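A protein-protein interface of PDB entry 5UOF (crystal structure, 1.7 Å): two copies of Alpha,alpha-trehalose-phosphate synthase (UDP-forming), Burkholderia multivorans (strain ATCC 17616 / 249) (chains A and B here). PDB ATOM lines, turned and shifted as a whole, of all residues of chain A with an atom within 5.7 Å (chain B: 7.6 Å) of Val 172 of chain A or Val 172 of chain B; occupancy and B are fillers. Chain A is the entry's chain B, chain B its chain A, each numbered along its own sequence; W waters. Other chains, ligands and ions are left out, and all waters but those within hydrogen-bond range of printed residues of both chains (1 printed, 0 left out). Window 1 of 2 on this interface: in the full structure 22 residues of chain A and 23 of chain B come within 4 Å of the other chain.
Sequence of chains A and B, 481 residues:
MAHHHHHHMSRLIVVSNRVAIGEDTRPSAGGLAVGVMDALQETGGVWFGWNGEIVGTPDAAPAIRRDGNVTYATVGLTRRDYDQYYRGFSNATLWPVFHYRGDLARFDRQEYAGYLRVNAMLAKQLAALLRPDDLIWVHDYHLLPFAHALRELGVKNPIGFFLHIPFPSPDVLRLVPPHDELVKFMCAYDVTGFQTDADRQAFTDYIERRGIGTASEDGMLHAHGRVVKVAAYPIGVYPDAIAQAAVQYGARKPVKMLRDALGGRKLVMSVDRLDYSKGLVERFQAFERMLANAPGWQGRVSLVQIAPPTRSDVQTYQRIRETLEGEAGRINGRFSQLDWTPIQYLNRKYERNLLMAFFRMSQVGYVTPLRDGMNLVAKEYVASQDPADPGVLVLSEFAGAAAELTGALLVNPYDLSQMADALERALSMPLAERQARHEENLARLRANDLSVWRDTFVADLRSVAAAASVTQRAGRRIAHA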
ATOM      1  N   VAL A  97      21.809 -34.394  -9.230  1.00  0.00           N
ATOM      2  CA  VAL A  97      21.132 -33.101  -9.195  1.00  0.00           C
ATOM      3  C   VAL A  97      21.419 -32.324 -10.471  1.00  0.00           C
ATOM      4  O   VAL A  97      20.515 -31.728 -11.064  1.00  0.00           O
ATOM      5  CB  VAL A  97      21.528 -32.294  -7.945  1.00  0.00           C
ATOM      6  CG1 VAL A  97      20.962 -30.887  -8.047  1.00  0.00           C
ATOM      7  CG2 VAL A  97      20.984 -32.960  -6.688  1.00  0.00           C
ATOM      8  N   TYR A 100      19.280 -33.221 -13.319  1.00  0.00           N
ATOM      9  CA  TYR A 100      17.849 -33.055 -13.107  1.00  0.00           C
ATOM     10  C   TYR A 100      17.198 -34.381 -12.693  1.00  0.00           C
ATOM     11  O   TYR A 100      16.041 -34.660 -13.027  1.00  0.00           O
ATOM     12  CB  TYR A 100      17.196 -32.444 -14.359  1.00  0.00           C
ATOM     13  CG  TYR A 100      17.509 -30.961 -14.524  1.00  0.00           C
ATOM     14  CD1 TYR A 100      18.743 -30.531 -14.990  1.00  0.00           C
ATOM     15  CD2 TYR A 100      16.564 -29.993 -14.208  1.00  0.00           C
ATOM     16  CE1 TYR A 100      19.032 -29.175 -15.134  1.00  0.00           C
ATOM     17  CE2 TYR A 100      16.842 -28.639 -14.334  1.00  0.00           C
ATOM     18  CZ  TYR A 100      18.076 -28.235 -14.802  1.00  0.00           C
ATOM     19  OH  TYR A 100      18.350 -26.895 -14.946  1.00  0.00           O
ATOM     20  N   PRO A 168      22.746 -26.830 -13.301  1.00  0.00           N
ATOM     21  CA  PRO A 168      21.313 -26.598 -13.099  1.00  0.00           C
ATOM     22  C   PRO A 168      20.986 -25.170 -12.661  1.00  0.00           C
ATOM     23  O   PRO A 168      21.797 -24.465 -12.057  1.00  0.00           O
ATOM     24  CB  PRO A 168      20.953 -27.607 -11.997  1.00  0.00           C
ATOM     25  CG  PRO A 168      22.207 -27.687 -11.159  1.00  0.00           C
ATOM     26  CD  PRO A 168      23.354 -27.607 -12.199  1.00  0.00           C
ATOM     27  N   SER A 169      19.751 -24.760 -12.963  1.00  0.00           N
ATOM     28  CA  SER A 169      19.242 -23.473 -12.511  1.00  0.00           C
ATOM     29  C   SER A 169      19.257 -23.408 -10.980  1.00  0.00           C
ATOM     30  O   SER A 169      19.293 -24.441 -10.310  1.00  0.00           O
ATOM     31  CB  SER A 169      17.825 -23.263 -13.056  1.00  0.00           C
ATOM     32  OG  SER A 169      16.941 -24.233 -12.508  1.00  0.00           O
ATOM     33  N   PRO A 170      19.232 -22.195 -10.402  1.00  0.00           N
ATOM     34  CA  PRO A 170      19.433 -22.079  -8.940  1.00  0.00           C
ATOM     35  C   PRO A 170      18.441 -22.878  -8.120  1.00  0.00           C
ATOM     36  O   PRO A 170      18.813 -23.459  -7.096  1.00  0.00           O
ATOM     37  CB  PRO A 170      19.298 -20.569  -8.687  1.00  0.00           C
ATOM     38  CG  PRO A 170      19.720 -19.940  -9.982  1.00  0.00           C
ATOM     39  CD  PRO A 170      19.262 -20.880 -11.073  1.00  0.00           C
ATOM     40  N   ASP A 171      17.179 -22.933  -8.547  1.00  0.00           N
ATOM     41  CA  ASP A 171      16.179 -23.708  -7.829  1.00  0.00           C
ATOM     42  C   ASP A 171      16.561 -25.188  -7.754  1.00  0.00           C
ATOM     43  O   ASP A 171      16.303 -25.856  -6.744  1.00  0.00           O
ATOM     44  CB  ASP A 171      14.809 -23.503  -8.497  1.00  0.00           C
ATOM     45  CG  ASP A 171      14.896 -23.340 -10.037  1.00  0.00           C
ATOM     46  OD1 ASP A 171      15.604 -22.438 -10.572  1.00  0.00           O
ATOM     47  OD2 ASP A 171      14.211 -24.130 -10.721  1.00  0.00           O
ATOM     48  N   VAL A 172      17.179 -25.709  -8.805  1.00  0.00           N
ATOM     49  CA  VAL A 172      17.540 -27.115  -8.835  1.00  0.00           C
ATOM     50  C   VAL A 172      18.884 -27.346  -8.153  1.00  0.00           C
ATOM     51  O   VAL A 172      19.058 -28.344  -7.452  1.00  0.00           O
ATOM     52  CB  VAL A 172      17.509 -27.593 -10.310  1.00  0.00           C
ATOM     53  CG1 VAL A 172      17.972 -29.040 -10.469  1.00  0.00           C
ATOM     54  CG2 VAL A 172      16.085 -27.439 -10.870  1.00  0.00           C
ATOM     55  N   LEU A 173      19.828 -26.406  -8.320  1.00  0.00           N
ATOM     56  CA  LEU A 173      21.137 -26.502  -7.669  1.00  0.00           C
ATOM     57  C   LEU A 173      21.006 -26.564  -6.155  1.00  0.00           C
ATOM     58  O   LEU A 173      21.801 -27.235  -5.481  1.00  0.00           O
ATOM     59  CB  LEU A 173      22.007 -25.303  -8.048  1.00  0.00           C
ATOM     60  CG  LEU A 173      23.398 -25.265  -7.425  1.00  0.00           C
ATOM     61  CD1 LEU A 173      24.230 -26.397  -8.029  1.00  0.00           C
ATOM     62  CD2 LEU A 173      24.096 -23.927  -7.648  1.00  0.00           C
ATOM     63  N   ARG A 174      20.022 -25.866  -5.597  1.00  0.00           N
ATOM     64  CA  ARG A 174      19.884 -25.824  -4.142  1.00  0.00           C
ATOM     65  C   ARG A 174      19.518 -27.173  -3.542  1.00  0.00           C
ATOM     66  O   ARG A 174      19.599 -27.329  -2.320  1.00  0.00           O
ATOM     67  CB  ARG A 174      18.855 -24.766  -3.748  1.00  0.00           C
ATOM     68  CG  ARG A 174      19.386 -23.345  -3.916  1.00  0.00           C
ATOM     69  CD  ARG A 174      18.264 -22.351  -3.939  1.00  0.00           C
ATOM     70  NE  ARG A 174      17.497 -22.408  -2.709  1.00  0.00           N
ATOM     71  CZ  ARG A 174      16.194 -22.175  -2.630  1.00  0.00           C
ATOM     72  NH1 ARG A 174      15.500 -21.888  -3.728  1.00  0.00           N
ATOM     73  NH2 ARG A 174      15.588 -22.246  -1.454  1.00  0.00           N
ATOM     74  N   LEU A 175      19.150 -28.156  -4.362  1.00  0.00           N
ATOM     75  CA  LEU A 175      19.004 -29.518  -3.867  1.00  0.00           C
ATOM     76  C   LEU A 175      20.326 -30.083  -3.360  1.00  0.00           C
ATOM     77  O   LEU A 175      20.321 -31.079  -2.627  1.00  0.00           O
ATOM     78  CB  LEU A 175      18.439 -30.430  -4.960  1.00  0.00           C
ATOM     79  CG  LEU A 175      16.937 -30.401  -5.276  1.00  0.00           C
ATOM     80  CD1 LEU A 175      16.323 -31.746  -4.951  1.00  0.00           C
ATOM     81  CD2 LEU A 175      16.197 -29.305  -4.540  1.00  0.00           C
ATOM     82  N   VAL A 176      21.451 -29.501  -3.765  1.00  0.00           N
ATOM     83  CA  VAL A 176      22.761 -29.857  -3.223  1.00  0.00           C
ATOM     84  C   VAL A 176      23.007 -28.979  -1.996  1.00  0.00           C
ATOM     85  O   VAL A 176      23.182 -27.763  -2.155  1.00  0.00           O
ATOM     86  CB  VAL A 176      23.868 -29.648  -4.262  1.00  0.00           C
ATOM     87  CG1 VAL A 176      25.242 -29.934  -3.626  1.00  0.00           C
ATOM     88  CG2 VAL A 176      23.630 -30.515  -5.499  1.00  0.00           C
ATOM     89  N   PRO B  96       3.090 -32.813 -10.259  1.00  0.00           N
ATOM     90  CA  PRO B  96       4.454 -33.237  -9.906  1.00  0.00           C
ATOM     91  C   PRO B  96       5.535 -32.347 -10.496  1.00  0.00           C
ATOM     92  O   PRO B  96       6.525 -32.062  -9.804  1.00  0.00           O
ATOM     93  CB  PRO B  96       4.533 -34.682 -10.428  1.00  0.00           C
ATOM     94  CG  PRO B  96       3.444 -34.787 -11.460  1.00  0.00           C
ATOM     95  CD  PRO B  96       2.352 -33.902 -10.930  1.00  0.00           C
ATOM     96  N   VAL B  97       5.391 -31.886 -11.744  1.00  0.00           N
ATOM     97  CA  VAL B  97       6.444 -31.055 -12.323  1.00  0.00           C
ATOM     98  C   VAL B  97       6.531 -29.719 -11.597  1.00  0.00           C
ATOM     99  O   VAL B  97       7.628 -29.230 -11.302  1.00  0.00           O
ATOM    100  CB  VAL B  97       6.228 -30.854 -13.833  1.00  0.00           C
ATOM    101  CG1 VAL B  97       7.220 -29.797 -14.350  1.00  0.00           C
ATOM    102  CG2 VAL B  97       6.420 -32.180 -14.583  1.00  0.00           C
ATOM    103  N   PHE B  98       5.380 -29.111 -11.284  1.00  0.00           N
ATOM    104  CA  PHE B  98       5.409 -27.824 -10.593  1.00  0.00           C
ATOM    105  C   PHE B  98       5.948 -27.952  -9.173  1.00  0.00           C
ATOM    106  O   PHE B  98       6.384 -26.948  -8.598  1.00  0.00           O
ATOM    107  CB  PHE B  98       4.016 -27.193 -10.548  1.00  0.00           C
ATOM    108  CG  PHE B  98       3.565 -26.562 -11.851  1.00  0.00           C
ATOM    109  CD1 PHE B  98       3.902 -27.112 -13.084  1.00  0.00           C
ATOM    110  CD2 PHE B  98       2.757 -25.434 -11.829  1.00  0.00           C
ATOM    111  CE1 PHE B  98       3.439 -26.536 -14.277  1.00  0.00           C
ATOM    112  CE2 PHE B  98       2.309 -24.843 -13.001  1.00  0.00           C
ATOM    113  CZ  PHE B  98       2.644 -25.403 -14.236  1.00  0.00           C
ATOM    114  N   HIS B  99       5.921 -29.154  -8.587  1.00  0.00           N
ATOM    115  CA  HIS B  99       6.572 -29.378  -7.296  1.00  0.00           C
ATOM    116  C   HIS B  99       7.965 -29.958  -7.462  1.00  0.00           C
ATOM    117  O   HIS B  99       8.505 -30.563  -6.520  1.00  0.00           O
ATOM    118  CB  HIS B  99       5.701 -30.257  -6.399  1.00  0.00           C
ATOM    119  CG  HIS B  99       4.465 -29.559  -5.920  1.00  0.00           C
ATOM    120  ND1 HIS B  99       3.330 -29.441  -6.695  1.00  0.00           N
ATOM    121  CD2 HIS B  99       4.203 -28.890  -4.767  1.00  0.00           C
ATOM    122  CE1 HIS B  99       2.417 -28.746  -6.036  1.00  0.00           C
ATOM    123  NE2 HIS B  99       2.922 -28.404  -4.862  1.00  0.00           N
ATOM    124  N   TYR B 100       8.561 -29.770  -8.641  1.00  0.00           N
ATOM    125  CA  TYR B 100       9.959 -30.121  -8.897  1.00  0.00           C
ATOM    126  C   TYR B 100      10.193 -31.627  -8.790  1.00  0.00           C
ATOM    127  O   TYR B 100      11.282 -32.088  -8.434  1.00  0.00           O
ATOM    128  CB  TYR B 100      10.904 -29.335  -7.979  1.00  0.00           C
ATOM    129  CG  TYR B 100      11.071 -27.905  -8.441  1.00  0.00           C
ATOM    130  CD1 TYR B 100      10.086 -26.960  -8.210  1.00  0.00           C
ATOM    131  CD2 TYR B 100      12.203 -27.505  -9.137  1.00  0.00           C
ATOM    132  CE1 TYR B 100      10.230 -25.650  -8.652  1.00  0.00           C
ATOM    133  CE2 TYR B 100      12.350 -26.213  -9.582  1.00  0.00           C
ATOM    134  CZ  TYR B 100      11.369 -25.282  -9.336  1.00  0.00           C
ATOM    135  OH  TYR B 100      11.527 -23.990  -9.777  1.00  0.00           O
ATOM    136  N   ARG B 101       9.170 -32.409  -9.133  1.00  0.00           N
ATOM    137  CA  ARG B 101       9.311 -33.856  -9.223  1.00  0.00           C
ATOM    138  C   ARG B 101       9.033 -34.337 -10.645  1.00  0.00           C
ATOM    139  O   ARG B 101       8.067 -35.067 -10.884  1.00  0.00           O
ATOM    140  CB  ARG B 101       8.391 -34.551  -8.215  1.00  0.00           C
ATOM    141  CG  ARG B 101       8.758 -34.335  -6.735  1.00  0.00           C
ATOM    142  CD  ARG B 101      10.127 -34.933  -6.377  1.00  0.00           C
ATOM    143  NE  ARG B 101      10.258 -36.359  -6.681  1.00  0.00           N
ATOM    144  CZ  ARG B 101      10.058 -37.342  -5.801  1.00  0.00           C
ATOM    145  NH1 ARG B 101       9.694 -37.068  -4.555  1.00  0.00           N
ATOM    146  NH2 ARG B 101      10.223 -38.606  -6.171  1.00  0.00           N
ATOM    147  N   GLY B 102       9.885 -33.948 -11.596  1.00  0.00           N
ATOM    148  CA  GLY B 102       9.748 -34.442 -12.957  1.00  0.00           C
ATOM    149  C   GLY B 102       9.768 -35.954 -13.062  1.00  0.00           C
ATOM    150  O   GLY B 102       9.173 -36.522 -13.981  1.00  0.00           O
ATOM    151  N   PHE B 167       5.365 -22.127  -9.217  1.00  0.00           N
ATOM    152  CA  PHE B 167       5.546 -22.138 -10.667  1.00  0.00           C
ATOM    153  C   PHE B 167       7.011 -22.413 -10.955  1.00  0.00           C
ATOM    154  O   PHE B 167       7.878 -21.630 -10.538  1.00  0.00           O
ATOM    155  CB  PHE B 167       5.104 -20.834 -11.328  1.00  0.00           C
ATOM    156  CG  PHE B 167       4.965 -20.957 -12.812  1.00  0.00           C
ATOM    157  CD1 PHE B 167       3.826 -21.522 -13.353  1.00  0.00           C
ATOM    158  CD2 PHE B 167       5.988 -20.554 -13.665  1.00  0.00           C
ATOM    159  CE1 PHE B 167       3.696 -21.674 -14.737  1.00  0.00           C
ATOM    160  CE2 PHE B 167       5.855 -20.694 -15.047  1.00  0.00           C
ATOM    161  CZ  PHE B 167       4.704 -21.244 -15.577  1.00  0.00           C
ATOM    162  N   PRO B 168       7.326 -23.517 -11.632  1.00  0.00           N
ATOM    163  CA  PRO B 168       8.725 -23.909 -11.801  1.00  0.00           C
ATOM    164  C   PRO B 168       9.463 -23.038 -12.806  1.00  0.00           C
ATOM    165  O   PRO B 168       8.876 -22.456 -13.721  1.00  0.00           O
ATOM    166  CB  PRO B 168       8.623 -25.355 -12.290  1.00  0.00           C
ATOM    167  CG  PRO B 168       7.332 -25.379 -13.073  1.00  0.00           C
ATOM    168  CD  PRO B 168       6.403 -24.411 -12.358  1.00  0.00           C
ATOM    169  N   SER B 169      10.786 -22.963 -12.616  1.00  0.00           N
ATOM    170  CA  SER B 169      11.651 -22.270 -13.562  1.00  0.00           C
ATOM    171  C   SER B 169      11.574 -22.935 -14.945  1.00  0.00           C
ATOM    172  O   SER B 169      11.163 -24.091 -15.066  1.00  0.00           O
ATOM    173  CB  SER B 169      13.085 -22.269 -13.040  1.00  0.00           C
ATOM    174  OG  SER B 169      13.526 -23.594 -12.830  1.00  0.00           O
ATOM    175  N   PRO B 170      11.942 -22.208 -16.009  1.00  0.00           N
ATOM    176  CA  PRO B 170      11.673 -22.730 -17.369  1.00  0.00           C
ATOM    177  C   PRO B 170      12.302 -24.084 -17.646  1.00  0.00           C
ATOM    178  O   PRO B 170      11.674 -24.930 -18.294  1.00  0.00           O
ATOM    179  CB  PRO B 170      12.249 -21.637 -18.282  1.00  0.00           C
ATOM    180  CG  PRO B 170      12.207 -20.387 -17.458  1.00  0.00           C
ATOM    181  CD  PRO B 170      12.434 -20.817 -16.039  1.00  0.00           C
ATOM    182  N   ASP B 171      13.527 -24.327 -17.159  1.00  0.00           N
ATOM    183  CA  ASP B 171      14.168 -25.619 -17.380  1.00  0.00           C
ATOM    184  C   ASP B 171      13.337 -26.763 -16.807  1.00  0.00           C
ATOM    185  O   ASP B 171      13.373 -27.881 -17.329  1.00  0.00           O
ATOM    186  CB  ASP B 171      15.570 -25.610 -16.763  1.00  0.00           C
ATOM    187  CG  ASP B 171      15.612 -24.935 -15.391  1.00  0.00           C
ATOM    188  OD1 ASP B 171      15.183 -23.756 -15.261  1.00  0.00           O
ATOM    189  OD2 ASP B 171      16.110 -25.587 -14.441  1.00  0.00           O
ATOM    190  N   VAL B 172      12.601 -26.508 -15.730  1.00  0.00           N
ATOM    191  CA  VAL B 172      11.804 -27.557 -15.108  1.00  0.00           C
ATOM    192  C   VAL B 172      10.402 -27.587 -15.700  1.00  0.00           C
ATOM    193  O   VAL B 172       9.830 -28.664 -15.898  1.00  0.00           O
ATOM    194  CB  VAL B 172      11.780 -27.340 -13.581  1.00  0.00           C
ATOM    195  CG1 VAL B 172      10.815 -28.311 -12.900  1.00  0.00           C
ATOM    196  CG2 VAL B 172      13.203 -27.513 -13.019  1.00  0.00           C
ATOM    197  N   LEU B 173       9.868 -26.412 -16.027  1.00  0.00           N
ATOM    198  CA  LEU B 173       8.556 -26.342 -16.677  1.00  0.00           C
ATOM    199  C   LEU B 173       8.527 -27.122 -17.988  1.00  0.00           C
ATOM    200  O   LEU B 173       7.493 -27.712 -18.342  1.00  0.00           O
ATOM    201  CB  LEU B 173       8.167 -24.889 -16.949  1.00  0.00           C
ATOM    202  CG  LEU B 173       6.781 -24.711 -17.591  1.00  0.00           C
ATOM    203  CD1 LEU B 173       5.665 -25.108 -16.615  1.00  0.00           C
ATOM    204  CD2 LEU B 173       6.562 -23.303 -18.116  1.00  0.00           C
ATOM    205  N   ARG B 174       9.644 -27.133 -18.727  1.00  0.00           N
ATOM    206  CA  ARG B 174       9.689 -27.815 -20.019  1.00  0.00           C
ATOM    207  C   ARG B 174       9.552 -29.327 -19.902  1.00  0.00           C
ATOM    208  O   ARG B 174       9.394 -29.997 -20.929  1.00  0.00           O
ATOM    209  CB  ARG B 174      10.981 -27.443 -20.750  1.00  0.00           C
ATOM    210  CG  ARG B 174      10.968 -26.010 -21.255  1.00  0.00           C
ATOM    211  CD  ARG B 174      12.337 -25.507 -21.721  1.00  0.00           C
ATOM    212  NE  ARG B 174      12.944 -26.367 -22.734  1.00  0.00           N
ATOM    213  CZ  ARG B 174      14.183 -26.843 -22.663  1.00  0.00           C
ATOM    214  NH1 ARG B 174      14.960 -26.530 -21.631  1.00  0.00           N
ATOM    215  NH2 ARG B 174      14.653 -27.618 -23.630  1.00  0.00           N
ATOM    216  N   LEU B 175       9.586 -29.878 -18.689  1.00  0.00           N
ATOM    217  CA  LEU B 175       9.261 -31.287 -18.514  1.00  0.00           C
ATOM    218  C   LEU B 175       7.792 -31.572 -18.800  1.00  0.00           C
ATOM    219  O   LEU B 175       7.435 -32.730 -19.032  1.00  0.00           O
ATOM    220  CB  LEU B 175       9.619 -31.735 -17.101  1.00  0.00           C
ATOM    221  CG  LEU B 175      11.111 -31.530 -16.804  1.00  0.00           C
ATOM    222  CD1 LEU B 175      11.438 -31.931 -15.374  1.00  0.00           C
ATOM    223  CD2 LEU B 175      11.956 -32.288 -17.783  1.00  0.00           C
ATOM    224  N   VAL B 176       6.940 -30.554 -18.762  1.00  0.00           N
ATOM    225  CA  VAL B 176       5.550 -30.675 -19.210  1.00  0.00           C
ATOM    226  C   VAL B 176       5.538 -30.487 -20.723  1.00  0.00           C
ATOM    227  O   VAL B 176       5.804 -29.377 -21.191  1.00  0.00           O
ATOM    228  CB  VAL B 176       4.648 -29.625 -18.535  1.00  0.00           C
ATOM    229  CG1 VAL B 176       3.219 -29.760 -19.045  1.00  0.00           C
ATOM    230  CG2 VAL B 176       4.683 -29.742 -17.014  1.00  0.00           C
ATOM    231  N   HIS B 179       4.172 -27.232 -22.465  1.00  0.00           N
ATOM    232  CA  HIS B 179       4.493 -26.044 -21.668  1.00  0.00           C
ATOM    233  C   HIS B 179       4.220 -24.751 -22.431  1.00  0.00           C
ATOM    234  O   HIS B 179       3.717 -23.783 -21.853  1.00  0.00           O
ATOM    235  CB  HIS B 179       5.957 -26.096 -21.220  1.00  0.00           C
ATOM    236  CG  HIS B 179       6.933 -26.284 -22.341  1.00  0.00           C
ATOM    237  ND1 HIS B 179       7.488 -25.229 -23.036  1.00  0.00           N
ATOM    238  CD2 HIS B 179       7.468 -27.408 -22.869  1.00  0.00           C
ATOM    239  CE1 HIS B 179       8.316 -25.700 -23.953  1.00  0.00           C
ATOM    240  NE2 HIS B 179       8.330 -27.018 -23.866  1.00  0.00           N
ATOM    241  N   ARG B 371       8.970 -29.182  -1.209  1.00  0.00           N
ATOM    242  CA  ARG B 371       8.545 -28.093  -2.075  1.00  0.00           C
ATOM    243  C   ARG B 371       7.094 -27.769  -1.744  1.00  0.00           C
ATOM    244  O   ARG B 371       6.270 -28.682  -1.616  1.00  0.00           O
ATOM    245  CB  ARG B 371       8.719 -28.498  -3.546  1.00  0.00           C
ATOM    246  CG  ARG B 371       8.328 -27.448  -4.571  1.00  0.00           C
ATOM    247  CD  ARG B 371       9.101 -26.156  -4.405  1.00  0.00           C
ATOM    248  NE  ARG B 371      10.503 -26.278  -4.804  1.00  0.00           N
ATOM    249  CZ  ARG B 371      11.248 -25.243  -5.186  1.00  0.00           C
ATOM    250  NH1 ARG B 371      10.711 -24.029  -5.242  1.00  0.00           N
ATOM    251  NH2 ARG B 371      12.514 -25.430  -5.549  1.00  0.00           N
ATOM    252  N   PHE B 398      12.344 -24.426   0.871  1.00  0.00           N
ATOM    253  CA  PHE B 398      11.596 -24.593  -0.372  1.00  0.00           C
ATOM    254  C   PHE B 398      10.100 -24.420  -0.186  1.00  0.00           C
ATOM    255  O   PHE B 398       9.331 -24.707  -1.122  1.00  0.00           O
ATOM    256  CB  PHE B 398      11.870 -25.959  -0.977  1.00  0.00           C
ATOM    257  CG  PHE B 398      13.332 -26.221  -1.250  1.00  0.00           C
ATOM    258  CD1 PHE B 398      13.997 -25.532  -2.247  1.00  0.00           C
ATOM    259  CD2 PHE B 398      14.025 -27.164  -0.506  1.00  0.00           C
ATOM    260  CE1 PHE B 398      15.341 -25.785  -2.508  1.00  0.00           C
ATOM    261  CE2 PHE B 398      15.366 -27.416  -0.754  1.00  0.00           C
ATOM    262  CZ  PHE B 398      16.018 -26.731  -1.751  1.00  0.00           C
HETATM  263  O   HOH W   1      13.842 -27.516  -5.909  1.00  0.00           O
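OD2 of Asp 171 of chain B is in hydrogen-bond range of OH of Tyr 100 of chain A, 2.6 Å away. OG of Ser 169 of chain B lies within hydrogen-bond range of OG of Ser 169 of chain A. The side-chain carboxylate of Asp 171 of chain B sits at hydrogen-bond distance from the side-chain hydroxyl of Ser 169 of chain A. OD1 of Asp 171 of chain A lies close to OG of Ser 169 of chain B. The side-chain carboxylate of Asp 171 of chain A sits at hydrogen-bond distance from the side-chain hydroxyl of Tyr 100 of chain B (2.8 Å).
The side-chain hydroxyl (OG) of Ser 169 of chain A lies within hydrogen-bond range of the side-chain carboxylate (OD1) of Asp 171 of chain A, at 3.0 Å. OH of Tyr 100 of chain A sits at hydrogen-bond distance from N of Ser 169 of chain A, 3.2 Å away. The side-chain hydroxyl (OG) of Ser 169 of chain B is in hydrogen-bond range of the side-chain carboxylate (OD1) of Asp 171 of chain B (2.9 Å). N of Ser 169 of chain B lies within hydrogen-bond range of OH of Tyr 100 of chain B (3.1 Å).
Asp 171 of chain A touches Arg 371 of chain B (O to NH2, 3.996 Å). Val 172 of chain A touches Val 172 of chain B (CG2 to CG2, 3.6 Å). Arg 174 of chain A touches Phe 398 of chain B. Phe 398 of chain B touches Leu 175 of chain A (CZ to CD2, 3.8 Å).
Of chain A, only Val 172 (3.6 Å) comes within 4 Å of Val 172 of chain B. Of the printed residues of chain A, Asp 171 of chain B touches Tyr 100 (2.6 Å) and Ser 169 (2.5 Å). Of the printed residues of chain A, Phe 398 of chain B touches Arg 174 (3.7 Å) and Leu 175 (3.8 Å). Of the printed residues of chain A, Ser 169 of chain B touches Ser 169 and Asp 171. Of the printed residues of chain B, Tyr 100 of chain A touches Asp 171 (2.6 Å). Of the printed residues of chain B, Asp 171 of chain A touches Tyr 100, Ser 169 and Arg 371. Pro 168 of chain B touches none of the printed residues of chain A. Phe 98 of chain B touches none of the printed residues of chain A. The nearest printed residue of chain B that does not touch Val 172 of chain A is Asp 171 of chain B (4.02 Å).
Of the 20 printed residues of chain B, 6 touch a printed residue of chain A. Hydrophobic or aromatic side chains of chain A that line the printed part of chain B: Tyr 100, Val 172 and Leu 175. Among the printed residues, no Asp or Glu carboxylate lies within 4 Å of a Lys or Arg side-chain nitrogen of the other chain.
Tyr 100 of chain A touches Asp 171 of chain B, and with the chains exchanged Asp 171 of chain A touches Tyr 100 of chain B. Ser 169 of chain B touches its own counterpart, Ser 169 of chain A. Ser 169 of chain A touches Asp 171 of chain B, and with the chains exchanged Asp 171 of chain A touches Ser 169 of chain B. Val 172 of chain A touches its own counterpart, Val 172 of chain B.
Water W1 lies within hydrogen-bond range of NH2 of Arg 371 of chain B (2.5 Å) and O of Asp 171 of chain A (3.1 Å).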
